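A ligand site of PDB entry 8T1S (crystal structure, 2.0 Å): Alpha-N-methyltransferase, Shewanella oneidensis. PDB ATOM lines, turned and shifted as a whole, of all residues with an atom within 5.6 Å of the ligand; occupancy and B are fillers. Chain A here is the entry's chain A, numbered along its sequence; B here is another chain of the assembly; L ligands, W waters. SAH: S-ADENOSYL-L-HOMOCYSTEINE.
The side-chain hydroxyl of Thr 235 lies within hydrogen-bond range of an oxygen (O2') of the ligand (2.7 Å). The backbone NH of Ala 207 sits at hydrogen-bond distance from a nitrogen (N1) of the ligand (2.7 Å). The backbone carbonyl oxygen (O) of Ala 207 is in hydrogen-bond range of a nitrogen (N6) of the ligand (2.9 Å). O of Pro 232 lies within hydrogen-bond range of O3' of the ligand. N of the ligand sits at hydrogen-bond distance from O of Val 97 (2.9 Å). The backbone NH of Ala 124 lies within hydrogen-bond range of an oxygen (OXT) of the ligand, at 2.9 Å. N of His 94 lies within hydrogen-bond range of O of the ligand (2.9 Å). N of the ligand is in hydrogen-bond range of O of His 94, at 3.0 Å. The backbone NH (N) of Gln 166 sits at hydrogen-bond distance from an oxygen (O2') of the ligand (2.9 Å). NE2 of Gln 166 sits close to SD of the ligand, 3.7 Å away. O of Ser 234 sits at hydrogen-bond distance from O2' of the ligand, 3.1 Å away.
The backbone carbonyl oxygen (O) of Phe 98 lies close to a sulfur (SD) of the ligand, 3.1 Å away. The backbone carbonyl oxygen (O) of Ile 233 lies close to a nitrogen (N3) of the ligand, 2.8 Å away. Leu 10 touches the ligand (CD1 to N6, 3.7 Å). Tyr 92 touches the ligand. Gly 93 touches the ligand (CA to O, 3.7 Å). Ser 123 touches the ligand (CB to O, 3.1 Å). Trp 165 touches the ligand. Tyr 205 touches the ligand. Glu 206 touches the ligand. IML 69 of chain B touches the ligand. Hydrophobic or aromatic side chains within 4 Å of the ligand: Leu 10, Tyr 92, His 94, Val 97, Phe 98, Ala 124, Trp 165, Tyr 205, Ala 207 and Ile 233. The nearest printed residue that does not touch the ligand is Leu 67 of chain B (4.03 Å).
Water W2 bridges the backbone carbonyl oxygen (O) of Tyr 92 (2.9 Å) and a nitrogen (N) of the ligand (2.9 Å). Water W1 lies within hydrogen-bond range of the side-chain amide oxygen of Asn 209 (2.9 Å) and a nitrogen (N6) of the ligand (3.1 Å).
The backbone NH of Tyr 205 lies within hydrogen-bond range of the backbone carbonyl oxygen of Thr 235, at 2.9 Å. The backbone NH (N) of Gly 96 sits at hydrogen-bond distance from a ring nitrogen (ND1) of His 94 (3.0 Å). OG of Ser 70 of chain B is in hydrogen-bond range of NE2 of Gln 166 (2.9 Å). The side-chain hydroxyl (OG) of Ser 70 of chain B lies within hydrogen-bond range of the backbone carbonyl oxygen (O) of Phe 98, 3.3 Å away. The side-chain carboxylate (OE2) of Glu 206 lies within hydrogen-bond range of the side-chain hydroxyl (OG) of Ser 234 (2.5 Å). OG of Ser 123 sits close to N of Glu 125 (3.4 Å). The backbone carbonyl oxygen (O) of Leu 67 of chain B lies within hydrogen-bond range of the side-chain hydroxyl (OH) of Tyr 92 (2.5 Å). The backbone carbonyl oxygen (O) of Leu 10 sits close to the side-chain amide oxygen (OD1) of Asn 209, at 3.1 Å.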
ATOM      1  N   LEU A  10     -14.924 -20.794   9.189  1.00  0.00           N
ATOM      2  CA  LEU A  10     -14.533 -21.467  10.420  1.00  0.00           C
ATOM      3  C   LEU A  10     -13.375 -22.424  10.157  1.00  0.00           C
ATOM      4  O   LEU A  10     -12.476 -22.546  10.990  1.00  0.00           O
ATOM      5  CB  LEU A  10     -15.740 -22.212  10.987  1.00  0.00           C
ATOM      6  CG  LEU A  10     -16.713 -21.365  11.799  1.00  0.00           C
ATOM      7  CD1 LEU A  10     -16.009 -20.679  12.963  1.00  0.00           C
ATOM      8  CD2 LEU A  10     -17.410 -20.337  10.918  1.00  0.00           C
ATOM      9  N   TYR A  92     -12.911 -14.159  11.470  1.00  0.00           N
ATOM     10  CA  TYR A  92     -13.313 -15.546  11.231  1.00  0.00           C
ATOM     11  C   TYR A  92     -14.828 -15.596  11.038  1.00  0.00           C
ATOM     12  O   TYR A  92     -15.547 -14.725  11.527  1.00  0.00           O
ATOM     13  CB  TYR A  92     -12.844 -16.454  12.374  1.00  0.00           C
ATOM     14  CG  TYR A  92     -13.644 -16.347  13.649  1.00  0.00           C
ATOM     15  CD1 TYR A  92     -13.401 -15.324  14.559  1.00  0.00           C
ATOM     16  CD2 TYR A  92     -14.653 -17.251  13.938  1.00  0.00           C
ATOM     17  CE1 TYR A  92     -14.142 -15.219  15.728  1.00  0.00           C
ATOM     18  CE2 TYR A  92     -15.394 -17.156  15.109  1.00  0.00           C
ATOM     19  CZ  TYR A  92     -15.141 -16.136  15.999  1.00  0.00           C
ATOM     20  OH  TYR A  92     -15.879 -16.033  17.155  1.00  0.00           O
ATOM     21  N   GLY A  93     -15.295 -16.616  10.316  1.00  0.00           N
ATOM     22  CA  GLY A  93     -16.692 -16.757   9.977  1.00  0.00           C
ATOM     23  C   GLY A  93     -17.172 -15.662   9.023  1.00  0.00           C
ATOM     24  O   GLY A  93     -16.513 -15.373   8.027  1.00  0.00           O
ATOM     25  N   HIS A  94     -18.327 -15.083   9.344  1.00  0.00           N
ATOM     26  CA  HIS A  94     -18.889 -13.964   8.597  1.00  0.00           C
ATOM     27  C   HIS A  94     -18.588 -12.684   9.385  1.00  0.00           C
ATOM     28  O   HIS A  94     -18.889 -12.592  10.580  1.00  0.00           O
ATOM     29  CB  HIS A  94     -20.384 -14.198   8.382  1.00  0.00           C
ATOM     30  CG  HIS A  94     -21.117 -13.149   7.602  1.00  0.00           C
ATOM     31  ND1 HIS A  94     -21.010 -11.799   7.835  1.00  0.00           N
ATOM     32  CD2 HIS A  94     -21.999 -13.284   6.602  1.00  0.00           C
ATOM     33  CE1 HIS A  94     -21.794 -11.144   6.991  1.00  0.00           C
ATOM     34  NE2 HIS A  94     -22.412 -12.024   6.239  1.00  0.00           N
ATOM     35  N   PRO A  95     -18.003 -11.645   8.744  1.00  0.00           N
ATOM     36  CA  PRO A  95     -17.473 -10.498   9.478  1.00  0.00           C
ATOM     37  C   PRO A  95     -18.545  -9.645  10.152  1.00  0.00           C
ATOM     38  O   PRO A  95     -18.233  -8.813  11.005  1.00  0.00           O
ATOM     39  CB  PRO A  95     -16.750  -9.689   8.384  1.00  0.00           C
ATOM     40  CG  PRO A  95     -17.481 -10.060   7.107  1.00  0.00           C
ATOM     41  CD  PRO A  95     -17.854 -11.517   7.281  1.00  0.00           C
ATOM     42  N   GLY A  96     -19.807  -9.851   9.754  1.00  0.00           N
ATOM     43  CA  GLY A  96     -20.904  -9.003  10.223  1.00  0.00           C
ATOM     44  C   GLY A  96     -21.962  -9.782  11.004  1.00  0.00           C
ATOM     45  O   GLY A  96     -23.020  -9.233  11.292  1.00  0.00           O
ATOM     46  N   VAL A  97     -21.662 -11.033  11.363  1.00  0.00           N
ATOM     47  CA  VAL A  97     -22.597 -11.864  12.117  1.00  0.00           C
ATOM     48  C   VAL A  97     -22.117 -11.952  13.565  1.00  0.00           C
ATOM     49  O   VAL A  97     -21.022 -12.458  13.831  1.00  0.00           O
ATOM     50  CB  VAL A  97     -22.764 -13.253  11.483  1.00  0.00           C
ATOM     51  CG1 VAL A  97     -23.634 -14.160  12.341  1.00  0.00           C
ATOM     52  CG2 VAL A  97     -23.329 -13.165  10.073  1.00  0.00           C
ATOM     53  N   PHE A  98     -22.950 -11.469  14.483  1.00  0.00           N
ATOM     54  CA  PHE A  98     -22.608 -11.349  15.889  1.00  0.00           C
ATOM     55  C   PHE A  98     -21.175 -10.835  16.018  1.00  0.00           C
ATOM     56  O   PHE A  98     -20.356 -11.414  16.724  1.00  0.00           O
ATOM     57  CB  PHE A  98     -22.787 -12.695  16.600  1.00  0.00           C
ATOM     58  CG  PHE A  98     -24.218 -13.100  16.814  1.00  0.00           C
ATOM     59  CD1 PHE A  98     -25.001 -13.540  15.750  1.00  0.00           C
ATOM     60  CD2 PHE A  98     -24.802 -13.031  18.068  1.00  0.00           C
ATOM     61  CE1 PHE A  98     -26.319 -13.915  15.942  1.00  0.00           C
ATOM     62  CE2 PHE A  98     -26.127 -13.395  18.265  1.00  0.00           C
ATOM     63  CZ  PHE A  98     -26.888 -13.837  17.198  1.00  0.00           C
ATOM     64  N   ALA A  99     -20.907  -9.715  15.335  1.00  0.00           N
ATOM     65  CA  ALA A  99     -19.624  -9.046  15.383  1.00  0.00           C
ATOM     66  C   ALA A  99     -19.826  -7.569  15.046  1.00  0.00           C
ATOM     67  O   ALA A  99     -20.284  -7.231  13.959  1.00  0.00           O
ATOM     68  CB  ALA A  99     -18.664  -9.704  14.415  1.00  0.00           C
ATOM     69  N   ILE A 122     -18.879 -17.371   5.509  1.00  0.00           N
ATOM     70  CA  ILE A 122     -19.554 -18.555   6.021  1.00  0.00           C
ATOM     71  C   ILE A 122     -19.509 -18.522   7.548  1.00  0.00           C
ATOM     72  O   ILE A 122     -18.423 -18.588   8.131  1.00  0.00           O
ATOM     73  CB  ILE A 122     -18.913 -19.829   5.450  1.00  0.00           C
ATOM     74  CG1 ILE A 122     -19.046 -19.895   3.927  1.00  0.00           C
ATOM     75  CG2 ILE A 122     -19.501 -21.077   6.111  1.00  0.00           C
ATOM     76  CD1 ILE A 122     -18.194 -20.971   3.284  1.00  0.00           C
ATOM     77  N   SER A 123     -20.679 -18.409   8.176  1.00  0.00           N
ATOM     78  CA  SER A 123     -20.806 -18.259   9.616  1.00  0.00           C
ATOM     79  C   SER A 123     -20.939 -19.632  10.293  1.00  0.00           C
ATOM     80  O   SER A 123     -21.104 -20.641   9.623  1.00  0.00           O
ATOM     81  CB  SER A 123     -21.975 -17.375   9.962  1.00  0.00           C
ATOM     82  OG  SER A 123     -23.200 -18.055   9.723  1.00  0.00           O
ATOM     83  N   ALA A 124     -20.887 -19.626  11.630  1.00  0.00           N
ATOM     84  CA  ALA A 124     -21.041 -20.837  12.418  1.00  0.00           C
ATOM     85  C   ALA A 124     -22.438 -21.419  12.215  1.00  0.00           C
ATOM     86  O   ALA A 124     -22.634 -22.637  12.279  1.00  0.00           O
ATOM     87  CB  ALA A 124     -20.780 -20.545  13.868  1.00  0.00           C
ATOM     88  N   GLU A 125     -23.411 -20.529  11.974  1.00  0.00           N
ATOM     89  CA  GLU A 125     -24.787 -20.927  11.713  1.00  0.00           C
ATOM     90  C   GLU A 125     -24.842 -21.706  10.399  1.00  0.00           C
ATOM     91  O   GLU A 125     -25.556 -22.706  10.291  1.00  0.00           O
ATOM     92  CB  GLU A 125     -25.668 -19.685  11.668  1.00  0.00           C
ATOM     93  CG  GLU A 125     -27.107 -19.969  11.265  1.00  0.00           C
ATOM     94  CD  GLU A 125     -27.969 -18.714  11.143  1.00  0.00           C
ATOM     95  OE1 GLU A 125     -28.083 -17.988  12.148  1.00  0.00           O
ATOM     96  OE2 GLU A 125     -28.501 -18.473  10.039  1.00  0.00           O
ATOM     97  N   LEU A 164     -29.026 -20.054  20.571  1.00  0.00           N
ATOM     98  CA  LEU A 164     -28.514 -19.088  21.521  1.00  0.00           C
ATOM     99  C   LEU A 164     -26.995 -18.999  21.351  1.00  0.00           C
ATOM    100  O   LEU A 164     -26.279 -19.956  21.646  1.00  0.00           O
ATOM    101  CB  LEU A 164     -28.878 -19.515  22.950  1.00  0.00           C
ATOM    102  CG  LEU A 164     -30.372 -19.513  23.273  1.00  0.00           C
ATOM    103  CD1 LEU A 164     -30.601 -19.715  24.758  1.00  0.00           C
ATOM    104  CD2 LEU A 164     -31.040 -18.232  22.811  1.00  0.00           C
ATOM    105  N   TRP A 165     -26.528 -17.847  20.868  1.00  0.00           N
ATOM    106  CA  TRP A 165     -25.106 -17.614  20.641  1.00  0.00           C
ATOM    107  C   TRP A 165     -24.463 -17.114  21.929  1.00  0.00           C
ATOM    108  O   TRP A 165     -25.125 -16.510  22.768  1.00  0.00           O
ATOM    109  CB  TRP A 165     -24.895 -16.598  19.506  1.00  0.00           C
ATOM    110  CG  TRP A 165     -25.484 -16.984  18.187  1.00  0.00           C
ATOM    111  CD1 TRP A 165     -26.788 -17.287  17.922  1.00  0.00           C
ATOM    112  CD2 TRP A 165     -24.785 -17.072  16.924  1.00  0.00           C
ATOM    113  NE1 TRP A 165     -26.943 -17.567  16.581  1.00  0.00           N
ATOM    114  CE2 TRP A 165     -25.737 -17.441  15.957  1.00  0.00           C
ATOM    115  CE3 TRP A 165     -23.455 -16.865  16.541  1.00  0.00           C
ATOM    116  CZ2 TRP A 165     -25.397 -17.619  14.611  1.00  0.00           C
ATOM    117  CZ3 TRP A 165     -23.124 -17.041  15.215  1.00  0.00           C
ATOM    118  CH2 TRP A 165     -24.080 -17.418  14.263  1.00  0.00           C
ATOM    119  N   GLN A 166     -23.150 -17.367  22.054  1.00  0.00           N
ATOM    120  CA  GLN A 166     -22.370 -16.910  23.194  1.00  0.00           C
ATOM    121  C   GLN A 166     -22.984 -17.439  24.487  1.00  0.00           C
ATOM    122  O   GLN A 166     -23.069 -16.726  25.484  1.00  0.00           O
ATOM    123  CB  GLN A 166     -22.283 -15.378  23.177  1.00  0.00           C
ATOM    124  CG  GLN A 166     -21.571 -14.831  21.949  1.00  0.00           C
ATOM    125  CD  GLN A 166     -21.310 -13.348  21.992  1.00  0.00           C
ATOM    126  OE1 GLN A 166     -21.734 -12.646  22.902  1.00  0.00           O
ATOM    127  NE2 GLN A 166     -20.600 -12.864  20.977  1.00  0.00           N
ATOM    128  N   ILE A 167     -23.370 -18.720  24.455  1.00  0.00           N
ATOM    129  CA  ILE A 167     -24.004 -19.361  25.604  1.00  0.00           C
ATOM    130  C   ILE A 167     -23.004 -19.422  26.770  1.00  0.00           C
ATOM    131  O   ILE A 167     -23.415 -19.476  27.926  1.00  0.00           O
ATOM    132  CB  ILE A 167     -24.509 -20.772  25.230  1.00  0.00           C
ATOM    133  CG1 ILE A 167     -25.340 -21.399  26.361  1.00  0.00           C
ATOM    134  CG2 ILE A 167     -23.365 -21.681  24.802  1.00  0.00           C
ATOM    135  CD1 ILE A 167     -26.570 -20.607  26.743  1.00  0.00           C
ATOM    136  N   TYR A 205     -23.216 -27.256  20.109  1.00  0.00           N
ATOM    137  CA  TYR A 205     -22.578 -27.393  18.805  1.00  0.00           C
ATOM    138  C   TYR A 205     -21.298 -26.581  18.752  1.00  0.00           C
ATOM    139  O   TYR A 205     -21.269 -25.421  19.171  1.00  0.00           O
ATOM    140  CB  TYR A 205     -23.524 -26.951  17.676  1.00  0.00           C
ATOM    141  CG  TYR A 205     -22.872 -26.892  16.319  1.00  0.00           C
ATOM    142  CD1 TYR A 205     -22.464 -28.054  15.680  1.00  0.00           C
ATOM    143  CD2 TYR A 205     -22.609 -25.686  15.699  1.00  0.00           C
ATOM    144  CE1 TYR A 205     -21.841 -28.024  14.444  1.00  0.00           C
ATOM    145  CE2 TYR A 205     -21.985 -25.636  14.461  1.00  0.00           C
ATOM    146  CZ  TYR A 205     -21.594 -26.805  13.834  1.00  0.00           C
ATOM    147  OH  TYR A 205     -20.978 -26.764  12.603  1.00  0.00           O
ATOM    148  N   GLU A 206     -20.237 -27.192  18.205  1.00  0.00           N
ATOM    149  CA  GLU A 206     -19.000 -26.496  17.927  1.00  0.00           C
ATOM    150  C   GLU A 206     -18.479 -26.942  16.555  1.00  0.00           C
ATOM    151  O   GLU A 206     -18.103 -28.102  16.385  1.00  0.00           O
ATOM    152  CB  GLU A 206     -17.949 -26.759  19.012  1.00  0.00           C
ATOM    153  CG  GLU A 206     -18.339 -26.193  20.371  1.00  0.00           C
ATOM    154  CD  GLU A 206     -17.403 -26.585  21.494  1.00  0.00           C
ATOM    155  OE1 GLU A 206     -16.400 -27.279  21.226  1.00  0.00           O
ATOM    156  OE2 GLU A 206     -17.687 -26.215  22.658  1.00  0.00           O
ATOM    157  N   ALA A 207     -18.482 -26.014  15.604  1.00  0.00           N
ATOM    158  CA  ALA A 207     -17.922 -26.278  14.285  1.00  0.00           C
ATOM    159  C   ALA A 207     -16.409 -26.425  14.410  1.00  0.00           C
ATOM    160  O   ALA A 207     -15.767 -25.707  15.174  1.00  0.00           O
ATOM    161  CB  ALA A 207     -18.280 -25.161  13.341  1.00  0.00           C
ATOM    162  N   ALA A 208     -15.852 -27.377  13.645  1.00  0.00           N
ATOM    163  CA  ALA A 208     -14.418 -27.609  13.644  1.00  0.00           C
ATOM    164  C   ALA A 208     -13.697 -26.433  12.975  1.00  0.00           C
ATOM    165  O   ALA A 208     -14.237 -25.801  12.077  1.00  0.00           O
ATOM    166  CB  ALA A 208     -14.109 -28.909  12.945  1.00  0.00           C
ATOM    167  N   ASN A 209     -12.461 -26.179  13.428  1.00  0.00           N
ATOM    168  CA  ASN A 209     -11.628 -25.134  12.854  1.00  0.00           C
ATOM    169  C   ASN A 209     -10.502 -25.763  12.023  1.00  0.00           C
ATOM    170  O   ASN A 209      -9.852 -25.073  11.246  1.00  0.00           O
ATOM    171  CB  ASN A 209     -11.060 -24.212  13.939  1.00  0.00           C
ATOM    172  CG  ASN A 209     -12.119 -23.425  14.678  1.00  0.00           C
ATOM    173  OD1 ASN A 209     -12.899 -22.690  14.064  1.00  0.00           O
ATOM    174  ND2 ASN A 209     -12.157 -23.555  15.985  1.00  0.00           N
ATOM    175  N   PRO A 232     -16.046 -20.701  24.658  1.00  0.00           N
ATOM    176  CA  PRO A 232     -16.482 -19.461  24.027  1.00  0.00           C
ATOM    177  C   PRO A 232     -17.097 -19.650  22.636  1.00  0.00           C
ATOM    178  O   PRO A 232     -17.933 -18.845  22.222  1.00  0.00           O
ATOM    179  CB  PRO A 232     -15.186 -18.634  23.926  1.00  0.00           C
ATOM    180  CG  PRO A 232     -14.315 -19.173  25.038  1.00  0.00           C
ATOM    181  CD  PRO A 232     -14.645 -20.641  25.120  1.00  0.00           C
ATOM    182  N   ILE A 233     -16.695 -20.716  21.937  1.00  0.00           N
ATOM    183  CA  ILE A 233     -17.150 -20.945  20.566  1.00  0.00           C
ATOM    184  C   ILE A 233     -18.405 -21.834  20.565  1.00  0.00           C
ATOM    185  O   ILE A 233     -18.909 -22.155  19.505  1.00  0.00           O
ATOM    186  CB  ILE A 233     -16.034 -21.576  19.706  1.00  0.00           C
ATOM    187  CG1 ILE A 233     -15.597 -22.934  20.240  1.00  0.00           C
ATOM    188  CG2 ILE A 233     -14.870 -20.613  19.549  1.00  0.00           C
ATOM    189  CD1 ILE A 233     -14.645 -23.678  19.329  1.00  0.00           C
ATOM    190  N   SER A 234     -18.886 -22.211  21.756  1.00  0.00           N
ATOM    191  CA  SER A 234     -20.074 -23.047  21.853  1.00  0.00           C
ATOM    192  C   SER A 234     -21.318 -22.272  21.415  1.00  0.00           C
ATOM    193  O   SER A 234     -21.464 -21.098  21.727  1.00  0.00           O
ATOM    194  CB  SER A 234     -20.240 -23.592  23.252  1.00  0.00           C
ATOM    195  OG  SER A 234     -19.146 -24.422  23.614  1.00  0.00           O
ATOM    196  N   THR A 235     -22.190 -22.961  20.671  1.00  0.00           N
ATOM    197  CA  THR A 235     -23.518 -22.453  20.339  1.00  0.00           C
ATOM    198  C   THR A 235     -24.551 -23.494  20.775  1.00  0.00           C
ATOM    199  O   THR A 235     -24.364 -24.684  20.557  1.00  0.00           O
ATOM    200  CB  THR A 235     -23.639 -22.134  18.846  1.00  0.00           C
ATOM    201  OG1 THR A 235     -22.770 -21.052  18.518  1.00  0.00           O
ATOM    202  CG2 THR A 235     -25.057 -21.777  18.435  1.00  0.00           C
ATOM    203  N   LEU B  67     -12.515 -15.137  21.152  1.00  0.00           N
ATOM    204  CA  LEU B  67     -13.113 -14.988  19.839  1.00  0.00           C
ATOM    205  C   LEU B  67     -14.494 -14.339  19.938  1.00  0.00           C
ATOM    206  O   LEU B  67     -15.273 -14.407  18.998  1.00  0.00           O
ATOM    207  CB  LEU B  67     -13.205 -16.374  19.187  1.00  0.00           C
ATOM    208  CG  LEU B  67     -11.871 -17.081  18.950  1.00  0.00           C
ATOM    209  CD1 LEU B  67     -12.062 -18.315  18.082  1.00  0.00           C
ATOM    210  CD2 LEU B  67     -10.856 -16.145  18.320  1.00  0.00           C
ATOM    211  N   VAL B  68     -14.780 -13.709  21.084  1.00  0.00           N
ATOM    212  CA  VAL B  68     -16.054 -13.029  21.291  1.00  0.00           C
ATOM    213  C   VAL B  68     -15.945 -11.615  20.728  1.00  0.00           C
ATOM    214  O   VAL B  68     -15.101 -10.837  21.193  1.00  0.00           O
ATOM    215  CB  VAL B  68     -16.456 -13.026  22.773  1.00  0.00           C
ATOM    216  CG1 VAL B  68     -17.667 -12.146  23.028  1.00  0.00           C
ATOM    217  CG2 VAL B  68     -16.709 -14.442  23.293  1.00  0.00           C
ATOM    218  N   IML B  69     -16.771 -11.232  19.723  1.00  0.00           N
ATOM    219  CA  IML B  69     -16.680  -9.880  19.113  1.00  0.00           C
ATOM    220  C   IML B  69     -17.976  -9.078  19.197  1.00  0.00           C
ATOM    221  O   IML B  69     -18.205  -8.182  18.386  1.00  0.00           O
ATOM    222  CB  IML B  69     -16.209 -10.009  17.646  1.00  0.00           C
ATOM    223  CN  IML B  69     -17.780 -12.115  19.170  1.00  0.00           C
ATOM    224  CG2 IML B  69     -15.700  -8.684  17.103  1.00  0.00           C
ATOM    225  CG1 IML B  69     -15.157 -11.110  17.488  1.00  0.00           C
ATOM    226  CD1 IML B  69     -15.045 -11.648  16.084  1.00  0.00           C
ATOM    227  N   SER B  70     -18.816  -9.394  20.190  1.00  0.00           N
ATOM    228  CA  SER B  70     -20.061  -8.685  20.412  1.00  0.00           C
ATOM    229  C   SER B  70     -20.528  -8.902  21.848  1.00  0.00           C
ATOM    230  O   SER B  70     -19.922  -9.682  22.590  1.00  0.00           O
ATOM    231  CB  SER B  70     -21.122  -9.107  19.426  1.00  0.00           C
ATOM    232  OG  SER B  70     -21.491 -10.461  19.620  1.00  0.00           O
HETATM  233  N   SAH L   1     -18.715 -14.020  13.178  1.00  0.00           N
HETATM  234  CA  SAH L   1     -18.807 -15.381  13.789  1.00  0.00           C
HETATM  235  CB  SAH L   1     -19.501 -15.315  15.149  1.00  0.00           C
HETATM  236  CG  SAH L   1     -18.794 -14.420  16.158  1.00  0.00           C
HETATM  237  SD  SAH L   1     -19.700 -14.241  17.718  1.00  0.00           S
HETATM  238  C   SAH L   1     -19.605 -16.293  12.848  1.00  0.00           C
HETATM  239  O   SAH L   1     -19.883 -15.852  11.714  1.00  0.00           O
HETATM  240  OXT SAH L   1     -19.921 -17.419  13.294  1.00  0.00           O
HETATM  241  C5' SAH L   1     -19.089 -15.648  18.672  1.00  0.00           C
HETATM  242  C4' SAH L   1     -20.118 -16.742  18.833  1.00  0.00           C
HETATM  243  O4' SAH L   1     -20.297 -17.427  17.570  1.00  0.00           O
HETATM  244  C3' SAH L   1     -19.758 -17.846  19.813  1.00  0.00           C
HETATM  245  O3' SAH L   1     -20.020 -17.463  21.158  1.00  0.00           O
HETATM  246  C2' SAH L   1     -20.691 -18.962  19.322  1.00  0.00           C
HETATM  247  O2' SAH L   1     -22.022 -18.784  19.732  1.00  0.00           O
HETATM  248  C1' SAH L   1     -20.530 -18.799  17.801  1.00  0.00           C
HETATM  249  N9  SAH L   1     -19.413 -19.573  17.278  1.00  0.00           N
HETATM  250  C8  SAH L   1     -18.148 -19.121  16.998  1.00  0.00           C
HETATM  251  N7  SAH L   1     -17.344 -20.064  16.572  1.00  0.00           N
HETATM  252  C5  SAH L   1     -18.121 -21.211  16.576  1.00  0.00           C
HETATM  253  C6  SAH L   1     -17.850 -22.549  16.227  1.00  0.00           C
HETATM  254  N6  SAH L   1     -16.667 -22.969  15.795  1.00  0.00           N
HETATM  255  N1  SAH L   1     -18.853 -23.447  16.352  1.00  0.00           N
HETATM  256  C2  SAH L   1     -20.038 -23.017  16.797  1.00  0.00           C
HETATM  257  N3  SAH L   1     -20.412 -21.790  17.162  1.00  0.00           N
HETATM  258  C4  SAH L   1     -19.401 -20.924  17.020  1.00  0.00           C
HETATM  259  O   HOH W   1     -14.407 -20.902  15.775  1.00  0.00           O
HETATM  260  O   HOH W   2     -16.102 -12.893  13.668  1.00  0.00           O
